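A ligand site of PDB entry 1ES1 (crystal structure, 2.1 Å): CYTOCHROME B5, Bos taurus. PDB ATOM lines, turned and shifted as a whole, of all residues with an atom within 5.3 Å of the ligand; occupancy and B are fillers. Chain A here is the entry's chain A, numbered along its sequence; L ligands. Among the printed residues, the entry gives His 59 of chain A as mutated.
Residues that only touch the ligand: Leu 30 (3.3 Å), Phe 33 (3.5 Å), Pro 38 (3.7 Å), Gly 39 (3.6 Å), Val 43 (3.7 Å), Leu 44 (3.5 Å), Gln 47 (3.6 Å), Asn 55 (3.4 Å), Phe 56 (3.6 Å), His 59 (3.5 Å), Ala 65 (3.4 Å) and Ser 69 (3.7 Å). Hydrophobic or aromatic side chains that line the ligand: Leu 30, Phe 33, His 37, Pro 38, Val 43, Leu 44, Phe 56, His 59, His 61 and Ala 65. 15 residues have an atom within 4 Å of the ligand: Leu 30, Phe 33, His 37, Pro 38, Gly 39, Val 43, Leu 44, Gln 47, Asn 55, Phe 56, His 59, His 61, Ser 62, Ala 65 and Ser 69. The nearest printed residue that does not touch the ligand is Ala 52 (4.2 Å).
A ring nitrogen (NE2) of His 61 is bound to an iron atom (FE1) of the ligand (2.1 Å). An iron atom (FE1) of the ligand is bound by a ring nitrogen (NE2) of His 37 (2.1 Å). An oxygen (O1) of the ligand is in hydrogen-bond range of the side-chain hydroxyl (OG) of Ser 62, at 2.5 Å. The backbone NH (N) of Ser 62 is in hydrogen-bond range of an oxygen (O2) of the ligand, at 3.0 Å.
The side-chain hydroxyl (OG) of Ser 62 sits at hydrogen-bond distance from the backbone NH (N) of Ala 65 (3.5 Å). The backbone carbonyl oxygen (O) of Asn 55 lies within hydrogen-bond range of a ring nitrogen (ND1) of His 59 (2.7 Å). The backbone carbonyl oxygen of Phe 56 is in hydrogen-bond range of a ring nitrogen (ND1) of His 61, at 3.1 Å.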
ATOM      1  N   LEU A  21      -4.404   5.652 -27.657  1.00  0.00           N
ATOM      2  CA  LEU A  21      -3.055   6.175 -27.780  1.00  0.00           C
ATOM      3  C   LEU A  21      -2.221   5.715 -26.586  1.00  0.00           C
ATOM      4  O   LEU A  21      -2.760   5.242 -25.589  1.00  0.00           O
ATOM      5  CB  LEU A  21      -3.046   7.697 -27.928  1.00  0.00           C
ATOM      6  CG  LEU A  21      -3.951   8.598 -27.105  1.00  0.00           C
ATOM      7  CD1 LEU A  21      -3.362   8.789 -25.721  1.00  0.00           C
ATOM      8  CD2 LEU A  21      -4.069   9.935 -27.828  1.00  0.00           C
ATOM      9  N   LEU A  23       0.838   6.488 -23.700  1.00  0.00           N
ATOM     10  CA  LEU A  23       1.516   7.507 -22.919  1.00  0.00           C
ATOM     11  C   LEU A  23       2.294   6.756 -21.837  1.00  0.00           C
ATOM     12  O   LEU A  23       1.700   6.053 -21.031  1.00  0.00           O
ATOM     13  CB  LEU A  23       0.520   8.455 -22.232  1.00  0.00           C
ATOM     14  CG  LEU A  23      -0.485   9.259 -23.060  1.00  0.00           C
ATOM     15  CD1 LEU A  23      -1.338  10.112 -22.112  1.00  0.00           C
ATOM     16  CD2 LEU A  23       0.244  10.127 -24.057  1.00  0.00           C
ATOM     17  N   TYR A  28      -4.371   4.239 -23.495  1.00  0.00           N
ATOM     18  CA  TYR A  28      -5.553   5.014 -23.129  1.00  0.00           C
ATOM     19  C   TYR A  28      -6.628   5.014 -24.210  1.00  0.00           C
ATOM     20  O   TYR A  28      -6.334   5.252 -25.379  1.00  0.00           O
ATOM     21  CB  TYR A  28      -5.172   6.476 -22.840  1.00  0.00           C
ATOM     22  CG  TYR A  28      -4.163   6.655 -21.731  1.00  0.00           C
ATOM     23  CD1 TYR A  28      -2.830   6.325 -21.925  1.00  0.00           C
ATOM     24  CD2 TYR A  28      -4.550   7.152 -20.495  1.00  0.00           C
ATOM     25  CE1 TYR A  28      -1.897   6.473 -20.907  1.00  0.00           C
ATOM     26  CE2 TYR A  28      -3.615   7.312 -19.457  1.00  0.00           C
ATOM     27  CZ  TYR A  28      -2.295   6.963 -19.675  1.00  0.00           C
ATOM     28  OH  TYR A  28      -1.371   7.122 -18.673  1.00  0.00           O
ATOM     29  N   LEU A  30      -9.371   7.074 -25.449  1.00  0.00           N
ATOM     30  CA  LEU A  30      -9.887   8.421 -25.310  1.00  0.00           C
ATOM     31  C   LEU A  30     -11.101   8.733 -26.186  1.00  0.00           C
ATOM     32  O   LEU A  30     -11.493   9.883 -26.357  1.00  0.00           O
ATOM     33  CB  LEU A  30      -8.770   9.414 -25.601  1.00  0.00           C
ATOM     34  CG  LEU A  30      -7.543   9.253 -24.702  1.00  0.00           C
ATOM     35  CD1 LEU A  30      -6.488  10.264 -25.088  1.00  0.00           C
ATOM     36  CD2 LEU A  30      -7.956   9.426 -23.243  1.00  0.00           C
ATOM     37  N   PHE A  33     -13.510  11.030 -24.672  1.00  0.00           N
ATOM     38  CA  PHE A  33     -12.906  12.211 -24.062  1.00  0.00           C
ATOM     39  C   PHE A  33     -12.563  13.298 -25.102  1.00  0.00           C
ATOM     40  O   PHE A  33     -12.382  14.472 -24.758  1.00  0.00           O
ATOM     41  CB  PHE A  33     -11.635  11.785 -23.315  1.00  0.00           C
ATOM     42  CG  PHE A  33     -10.894  12.909 -22.656  1.00  0.00           C
ATOM     43  CD1 PHE A  33     -11.442  13.611 -21.588  1.00  0.00           C
ATOM     44  CD2 PHE A  33      -9.620  13.255 -23.090  1.00  0.00           C
ATOM     45  CE1 PHE A  33     -10.739  14.642 -20.964  1.00  0.00           C
ATOM     46  CE2 PHE A  33      -8.907  14.277 -22.472  1.00  0.00           C
ATOM     47  CZ  PHE A  33      -9.477  14.971 -21.408  1.00  0.00           C
ATOM     48  N   HIS A  37     -11.841  17.300 -24.031  1.00  0.00           N
ATOM     49  CA  HIS A  37     -10.442  17.693 -23.916  1.00  0.00           C
ATOM     50  C   HIS A  37     -10.206  19.197 -24.109  1.00  0.00           C
ATOM     51  O   HIS A  37     -10.379  19.722 -25.209  1.00  0.00           O
ATOM     52  CB  HIS A  37      -9.596  16.913 -24.924  1.00  0.00           C
ATOM     53  CG  HIS A  37      -8.144  17.239 -24.862  1.00  0.00           C
ATOM     54  ND1 HIS A  37      -7.386  17.601 -25.962  1.00  0.00           N
ATOM     55  CD2 HIS A  37      -7.290  17.241 -23.805  1.00  0.00           C
ATOM     56  CE1 HIS A  37      -6.130  17.800 -25.532  1.00  0.00           C
ATOM     57  NE2 HIS A  37      -6.036  17.597 -24.233  1.00  0.00           N
ATOM     58  N   PRO A  38      -9.801  19.895 -23.036  1.00  0.00           N
ATOM     59  CA  PRO A  38      -9.524  21.337 -23.079  1.00  0.00           C
ATOM     60  C   PRO A  38      -8.606  21.721 -24.221  1.00  0.00           C
ATOM     61  O   PRO A  38      -8.715  22.816 -24.766  1.00  0.00           O
ATOM     62  CB  PRO A  38      -8.891  21.599 -21.721  1.00  0.00           C
ATOM     63  CG  PRO A  38      -9.619  20.663 -20.825  1.00  0.00           C
ATOM     64  CD  PRO A  38      -9.656  19.387 -21.655  1.00  0.00           C
ATOM     65  N   GLY A  39      -7.715  20.817 -24.600  1.00  0.00           N
ATOM     66  CA  GLY A  39      -6.791  21.105 -25.684  1.00  0.00           C
ATOM     67  C   GLY A  39      -7.363  20.882 -27.076  1.00  0.00           C
ATOM     68  O   GLY A  39      -6.689  21.137 -28.066  1.00  0.00           O
ATOM     69  N   VAL A  43      -5.900  17.676 -31.861  1.00  0.00           N
ATOM     70  CA  VAL A  43      -4.572  17.338 -31.377  1.00  0.00           C
ATOM     71  C   VAL A  43      -4.501  15.886 -30.879  1.00  0.00           C
ATOM     72  O   VAL A  43      -3.432  15.276 -30.848  1.00  0.00           O
ATOM     73  CB  VAL A  43      -4.134  18.317 -30.246  1.00  0.00           C
ATOM     74  CG1 VAL A  43      -4.984  18.125 -29.007  1.00  0.00           C
ATOM     75  CG2 VAL A  43      -2.662  18.118 -29.933  1.00  0.00           C
ATOM     76  N   LEU A  44      -5.643  15.328 -30.505  1.00  0.00           N
ATOM     77  CA  LEU A  44      -5.698  13.946 -30.023  1.00  0.00           C
ATOM     78  C   LEU A  44      -5.876  12.964 -31.189  1.00  0.00           C
ATOM     79  O   LEU A  44      -5.295  11.880 -31.174  1.00  0.00           O
ATOM     80  CB  LEU A  44      -6.857  13.774 -29.032  1.00  0.00           C
ATOM     81  CG  LEU A  44      -6.768  14.565 -27.715  1.00  0.00           C
ATOM     82  CD1 LEU A  44      -8.008  14.328 -26.872  1.00  0.00           C
ATOM     83  CD2 LEU A  44      -5.517  14.136 -26.959  1.00  0.00           C
ATOM     84  N   GLN A  47      -2.664  11.925 -33.068  1.00  0.00           N
ATOM     85  CA  GLN A  47      -1.767  10.978 -32.412  1.00  0.00           C
ATOM     86  C   GLN A  47      -2.387   9.599 -32.263  1.00  0.00           C
ATOM     87  O   GLN A  47      -1.711   8.649 -31.870  1.00  0.00           O
ATOM     88  CB  GLN A  47      -1.384  11.491 -31.018  1.00  0.00           C
ATOM     89  CG  GLN A  47      -0.729  12.862 -31.008  1.00  0.00           C
ATOM     90  CD  GLN A  47       0.537  12.903 -31.843  1.00  0.00           C
ATOM     91  OE1 GLN A  47       1.353  11.982 -31.785  1.00  0.00           O
ATOM     92  NE2 GLN A  47       0.718  13.972 -32.602  1.00  0.00           N
ATOM     93  N   ALA A  52       2.070   8.903 -27.982  1.00  0.00           N
ATOM     94  CA  ALA A  52       1.992  10.367 -27.908  1.00  0.00           C
ATOM     95  C   ALA A  52       2.645  10.933 -26.644  1.00  0.00           C
ATOM     96  O   ALA A  52       2.322  12.042 -26.228  1.00  0.00           O
ATOM     97  CB  ALA A  52       0.548  10.819 -27.969  1.00  0.00           C
ATOM     98  N   ASN A  55       4.640  14.475 -27.085  1.00  0.00           N
ATOM     99  CA  ASN A  55       3.700  15.564 -27.299  1.00  0.00           C
ATOM    100  C   ASN A  55       2.951  15.901 -26.012  1.00  0.00           C
ATOM    101  O   ASN A  55       2.750  17.062 -25.680  1.00  0.00           O
ATOM    102  CB  ASN A  55       2.669  15.213 -28.374  1.00  0.00           C
ATOM    103  CG  ASN A  55       3.306  14.726 -29.649  1.00  0.00           C
ATOM    104  OD1 ASN A  55       3.780  13.592 -29.726  1.00  0.00           O
ATOM    105  ND2 ASN A  55       3.322  15.580 -30.661  1.00  0.00           N
ATOM    106  N   PHE A  56       2.529  14.859 -25.298  1.00  0.00           N
ATOM    107  CA  PHE A  56       1.808  15.039 -24.049  1.00  0.00           C
ATOM    108  C   PHE A  56       2.678  15.855 -23.087  1.00  0.00           C
ATOM    109  O   PHE A  56       2.234  16.866 -22.532  1.00  0.00           O
ATOM    110  CB  PHE A  56       1.498  13.669 -23.432  1.00  0.00           C
ATOM    111  CG  PHE A  56       0.769  13.732 -22.127  1.00  0.00           C
ATOM    112  CD1 PHE A  56      -0.562  14.147 -22.069  1.00  0.00           C
ATOM    113  CD2 PHE A  56       1.399  13.352 -20.933  1.00  0.00           C
ATOM    114  CE1 PHE A  56      -1.255  14.193 -20.857  1.00  0.00           C
ATOM    115  CE2 PHE A  56       0.716  13.392 -19.713  1.00  0.00           C
ATOM    116  CZ  PHE A  56      -0.617  13.809 -19.677  1.00  0.00           C
ATOM    117  N   HIS A  59       3.476  19.681 -23.927  1.00  0.00           N
ATOM    118  CA  HIS A  59       2.514  20.708 -23.544  1.00  0.00           C
ATOM    119  C   HIS A  59       2.420  20.818 -22.016  1.00  0.00           C
ATOM    120  O   HIS A  59       1.592  21.556 -21.493  1.00  0.00           O
ATOM    121  CB  HIS A  59       1.124  20.397 -24.114  1.00  0.00           C
ATOM    122  CG  HIS A  59       1.079  20.296 -25.615  1.00  0.00           C
ATOM    123  ND1 HIS A  59       1.073  19.086 -26.273  1.00  0.00           N
ATOM    124  CD2 HIS A  59       1.034  21.256 -26.561  1.00  0.00           C
ATOM    125  CE1 HIS A  59       1.020  19.309 -27.571  1.00  0.00           C
ATOM    126  NE2 HIS A  59       0.990  20.610 -27.775  1.00  0.00           N
ATOM    127  N   GLY A  60       3.263  20.066 -21.322  1.00  0.00           N
ATOM    128  CA  GLY A  60       3.289  20.078 -19.866  1.00  0.00           C
ATOM    129  C   GLY A  60       1.964  20.095 -19.113  1.00  0.00           C
ATOM    130  O   GLY A  60       1.571  21.130 -18.567  1.00  0.00           O
ATOM    131  N   HIS A  61       1.298  18.949 -19.066  1.00  0.00           N
ATOM    132  CA  HIS A  61       0.010  18.820 -18.368  1.00  0.00           C
ATOM    133  C   HIS A  61       0.097  18.940 -16.868  1.00  0.00           C
ATOM    134  O   HIS A  61       1.059  18.475 -16.254  1.00  0.00           O
ATOM    135  CB  HIS A  61      -0.644  17.493 -18.716  1.00  0.00           C
ATOM    136  CG  HIS A  61      -1.242  17.445 -20.082  1.00  0.00           C
ATOM    137  ND1 HIS A  61      -0.501  17.480 -21.243  1.00  0.00           N
ATOM    138  CD2 HIS A  61      -2.540  17.462 -20.472  1.00  0.00           C
ATOM    139  CE1 HIS A  61      -1.352  17.498 -22.276  1.00  0.00           C
ATOM    140  NE2 HIS A  61      -2.601  17.490 -21.856  1.00  0.00           N
ATOM    141  N   SER A  62      -0.930  19.534 -16.272  1.00  0.00           N
ATOM    142  CA  SER A  62      -0.999  19.744 -14.834  1.00  0.00           C
ATOM    143  C   SER A  62      -1.261  18.427 -14.101  1.00  0.00           C
ATOM    144  O   SER A  62      -1.581  17.420 -14.730  1.00  0.00           O
ATOM    145  CB  SER A  62      -2.117  20.734 -14.499  1.00  0.00           C
ATOM    146  OG  SER A  62      -3.393  20.208 -14.837  1.00  0.00           O
ATOM    147  N   ALA A  65      -4.786  17.048 -14.612  1.00  0.00           N
ATOM    148  CA  ALA A  65      -4.924  16.409 -15.917  1.00  0.00           C
ATOM    149  C   ALA A  65      -4.367  14.984 -15.881  1.00  0.00           C
ATOM    150  O   ALA A  65      -4.989  14.063 -16.411  1.00  0.00           O
ATOM    151  CB  ALA A  65      -4.200  17.229 -16.968  1.00  0.00           C
ATOM    152  N   LEU A  68      -6.601  12.690 -13.876  1.00  0.00           N
ATOM    153  CA  LEU A  68      -7.808  12.365 -14.642  1.00  0.00           C
ATOM    154  C   LEU A  68      -7.557  11.328 -15.732  1.00  0.00           C
ATOM    155  O   LEU A  68      -8.402  10.486 -15.992  1.00  0.00           O
ATOM    156  CB  LEU A  68      -8.380  13.636 -15.281  1.00  0.00           C
ATOM    157  CG  LEU A  68      -9.649  13.462 -16.130  1.00  0.00           C
ATOM    158  CD1 LEU A  68     -10.758  12.842 -15.301  1.00  0.00           C
ATOM    159  CD2 LEU A  68     -10.081  14.812 -16.672  1.00  0.00           C
ATOM    160  N   SER A  69      -6.382  11.393 -16.365  1.00  0.00           N
ATOM    161  CA  SER A  69      -6.041  10.462 -17.448  1.00  0.00           C
ATOM    162  C   SER A  69      -6.116   8.992 -17.032  1.00  0.00           C
ATOM    163  O   SER A  69      -6.492   8.137 -17.838  1.00  0.00           O
ATOM    164  CB  SER A  69      -4.633  10.778 -17.969  1.00  0.00           C
ATOM    165  OG  SER A  69      -3.634  10.488 -16.999  1.00  0.00           O
ATOM    166  N   PHE A  72      -8.913   6.585 -17.999  1.00  0.00           N
ATOM    167  CA  PHE A  72      -9.012   6.089 -19.369  1.00  0.00           C
ATOM    168  C   PHE A  72      -8.026   4.977 -19.734  1.00  0.00           C
ATOM    169  O   PHE A  72      -7.994   4.512 -20.871  1.00  0.00           O
ATOM    170  CB  PHE A  72      -8.853   7.249 -20.365  1.00  0.00           C
ATOM    171  CG  PHE A  72      -9.856   8.359 -20.166  1.00  0.00           C
ATOM    172  CD1 PHE A  72     -11.197   8.159 -20.467  1.00  0.00           C
ATOM    173  CD2 PHE A  72      -9.463   9.582 -19.649  1.00  0.00           C
ATOM    174  CE1 PHE A  72     -12.146   9.174 -20.256  1.00  0.00           C
ATOM    175  CE2 PHE A  72     -10.391  10.613 -19.428  1.00  0.00           C
ATOM    176  CZ  PHE A  72     -11.733  10.404 -19.735  1.00  0.00           C
HETATM  177  C1  LIG L   1      -4.662  20.820 -22.205  1.00  0.00           C
HETATM  178  C2  LIG L   1      -6.276  16.753 -20.202  1.00  0.00           C
HETATM  179  C3  LIG L   1      -3.877  14.164 -23.488  1.00  0.00           C
HETATM  180  C4  LIG L   1      -2.490  18.257 -25.724  1.00  0.00           C
HETATM  181  C5  LIG L   1      -5.198  19.909 -21.303  1.00  0.00           C
HETATM  182  C6  LIG L   1      -5.866  20.282 -20.088  1.00  0.00           C
HETATM  183  C7  LIG L   1      -6.373  19.143 -19.564  1.00  0.00           C
HETATM  184  C8  LIG L   1      -5.997  18.065 -20.455  1.00  0.00           C
HETATM  185  C9  LIG L   1      -7.126  19.014 -18.250  1.00  0.00           C
HETATM  186  C10 LIG L   1      -5.959  21.657 -19.433  1.00  0.00           C
HETATM  187  C11 LIG L   1      -4.634  22.179 -18.886  1.00  0.00           C
HETATM  188  C12 LIG L   1      -3.988  21.205 -17.920  1.00  0.00           C
HETATM  189  O1  LIG L   1      -4.618  20.859 -16.903  1.00  0.00           O
HETATM  190  O2  LIG L   1      -2.847  20.775 -18.189  1.00  0.00           O
HETATM  191  C13 LIG L   1      -5.783  15.684 -20.957  1.00  0.00           C
HETATM  192  C14 LIG L   1      -5.932  14.303 -20.557  1.00  0.00           C
HETATM  193  C15 LIG L   1      -5.218  13.573 -21.453  1.00  0.00           C
HETATM  194  C16 LIG L   1      -4.683  14.517 -22.427  1.00  0.00           C
HETATM  195  C17 LIG L   1      -6.704  13.808 -19.317  1.00  0.00           C
HETATM  196  C18 LIG L   1      -4.871  12.244 -21.311  1.00  0.00           C
HETATM  197  C19 LIG L   1      -5.466  11.232 -22.040  1.00  0.00           C
HETATM  198  C20 LIG L   1      -3.251  15.060 -24.362  1.00  0.00           C
HETATM  199  C21 LIG L   1      -2.421  14.643 -25.474  1.00  0.00           C
HETATM  200  C22 LIG L   1      -2.051  15.776 -26.156  1.00  0.00           C
HETATM  201  C23 LIG L   1      -2.662  16.891 -25.420  1.00  0.00           C
HETATM  202  C24 LIG L   1      -2.165  13.183 -25.886  1.00  0.00           C
HETATM  203  C25 LIG L   1      -1.271  15.915 -27.300  1.00  0.00           C
HETATM  204  C26 LIG L   1      -0.706  14.887 -28.075  1.00  0.00           C
HETATM  205  C27 LIG L   1      -3.034  19.316 -24.964  1.00  0.00           C
HETATM  206  C28 LIG L   1      -2.951  20.731 -25.295  1.00  0.00           C
HETATM  207  C29 LIG L   1      -3.532  21.433 -24.298  1.00  0.00           C
HETATM  208  C30 LIG L   1      -4.011  20.461 -23.364  1.00  0.00           C
HETATM  209  C31 LIG L   1      -2.441  21.356 -26.587  1.00  0.00           C
HETATM  210  C32 LIG L   1      -3.614  22.960 -24.174  1.00  0.00           C
HETATM  211  C33 LIG L   1      -2.289  23.515 -23.700  1.00  0.00           C
HETATM  212  C34 LIG L   1      -2.211  25.029 -23.828  1.00  0.00           C
HETATM  213  O3  LIG L   1      -1.125  25.592 -23.575  1.00  0.00           O
HETATM  214  O4  LIG L   1      -3.241  25.656 -24.178  1.00  0.00           O
HETATM  215  N1  LIG L   1      -5.239  18.531 -21.513  1.00  0.00           N
HETATM  216  N2  LIG L   1      -5.003  15.826 -22.087  1.00  0.00           N
HETATM  217  N3  LIG L   1      -3.397  16.433 -24.322  1.00  0.00           N
HETATM  218  N4  LIG L   1      -3.753  19.165 -23.792  1.00  0.00           N
HETATM  219 FE1  LIG L   1      -4.368  17.504 -22.945  1.00  0.00          FE
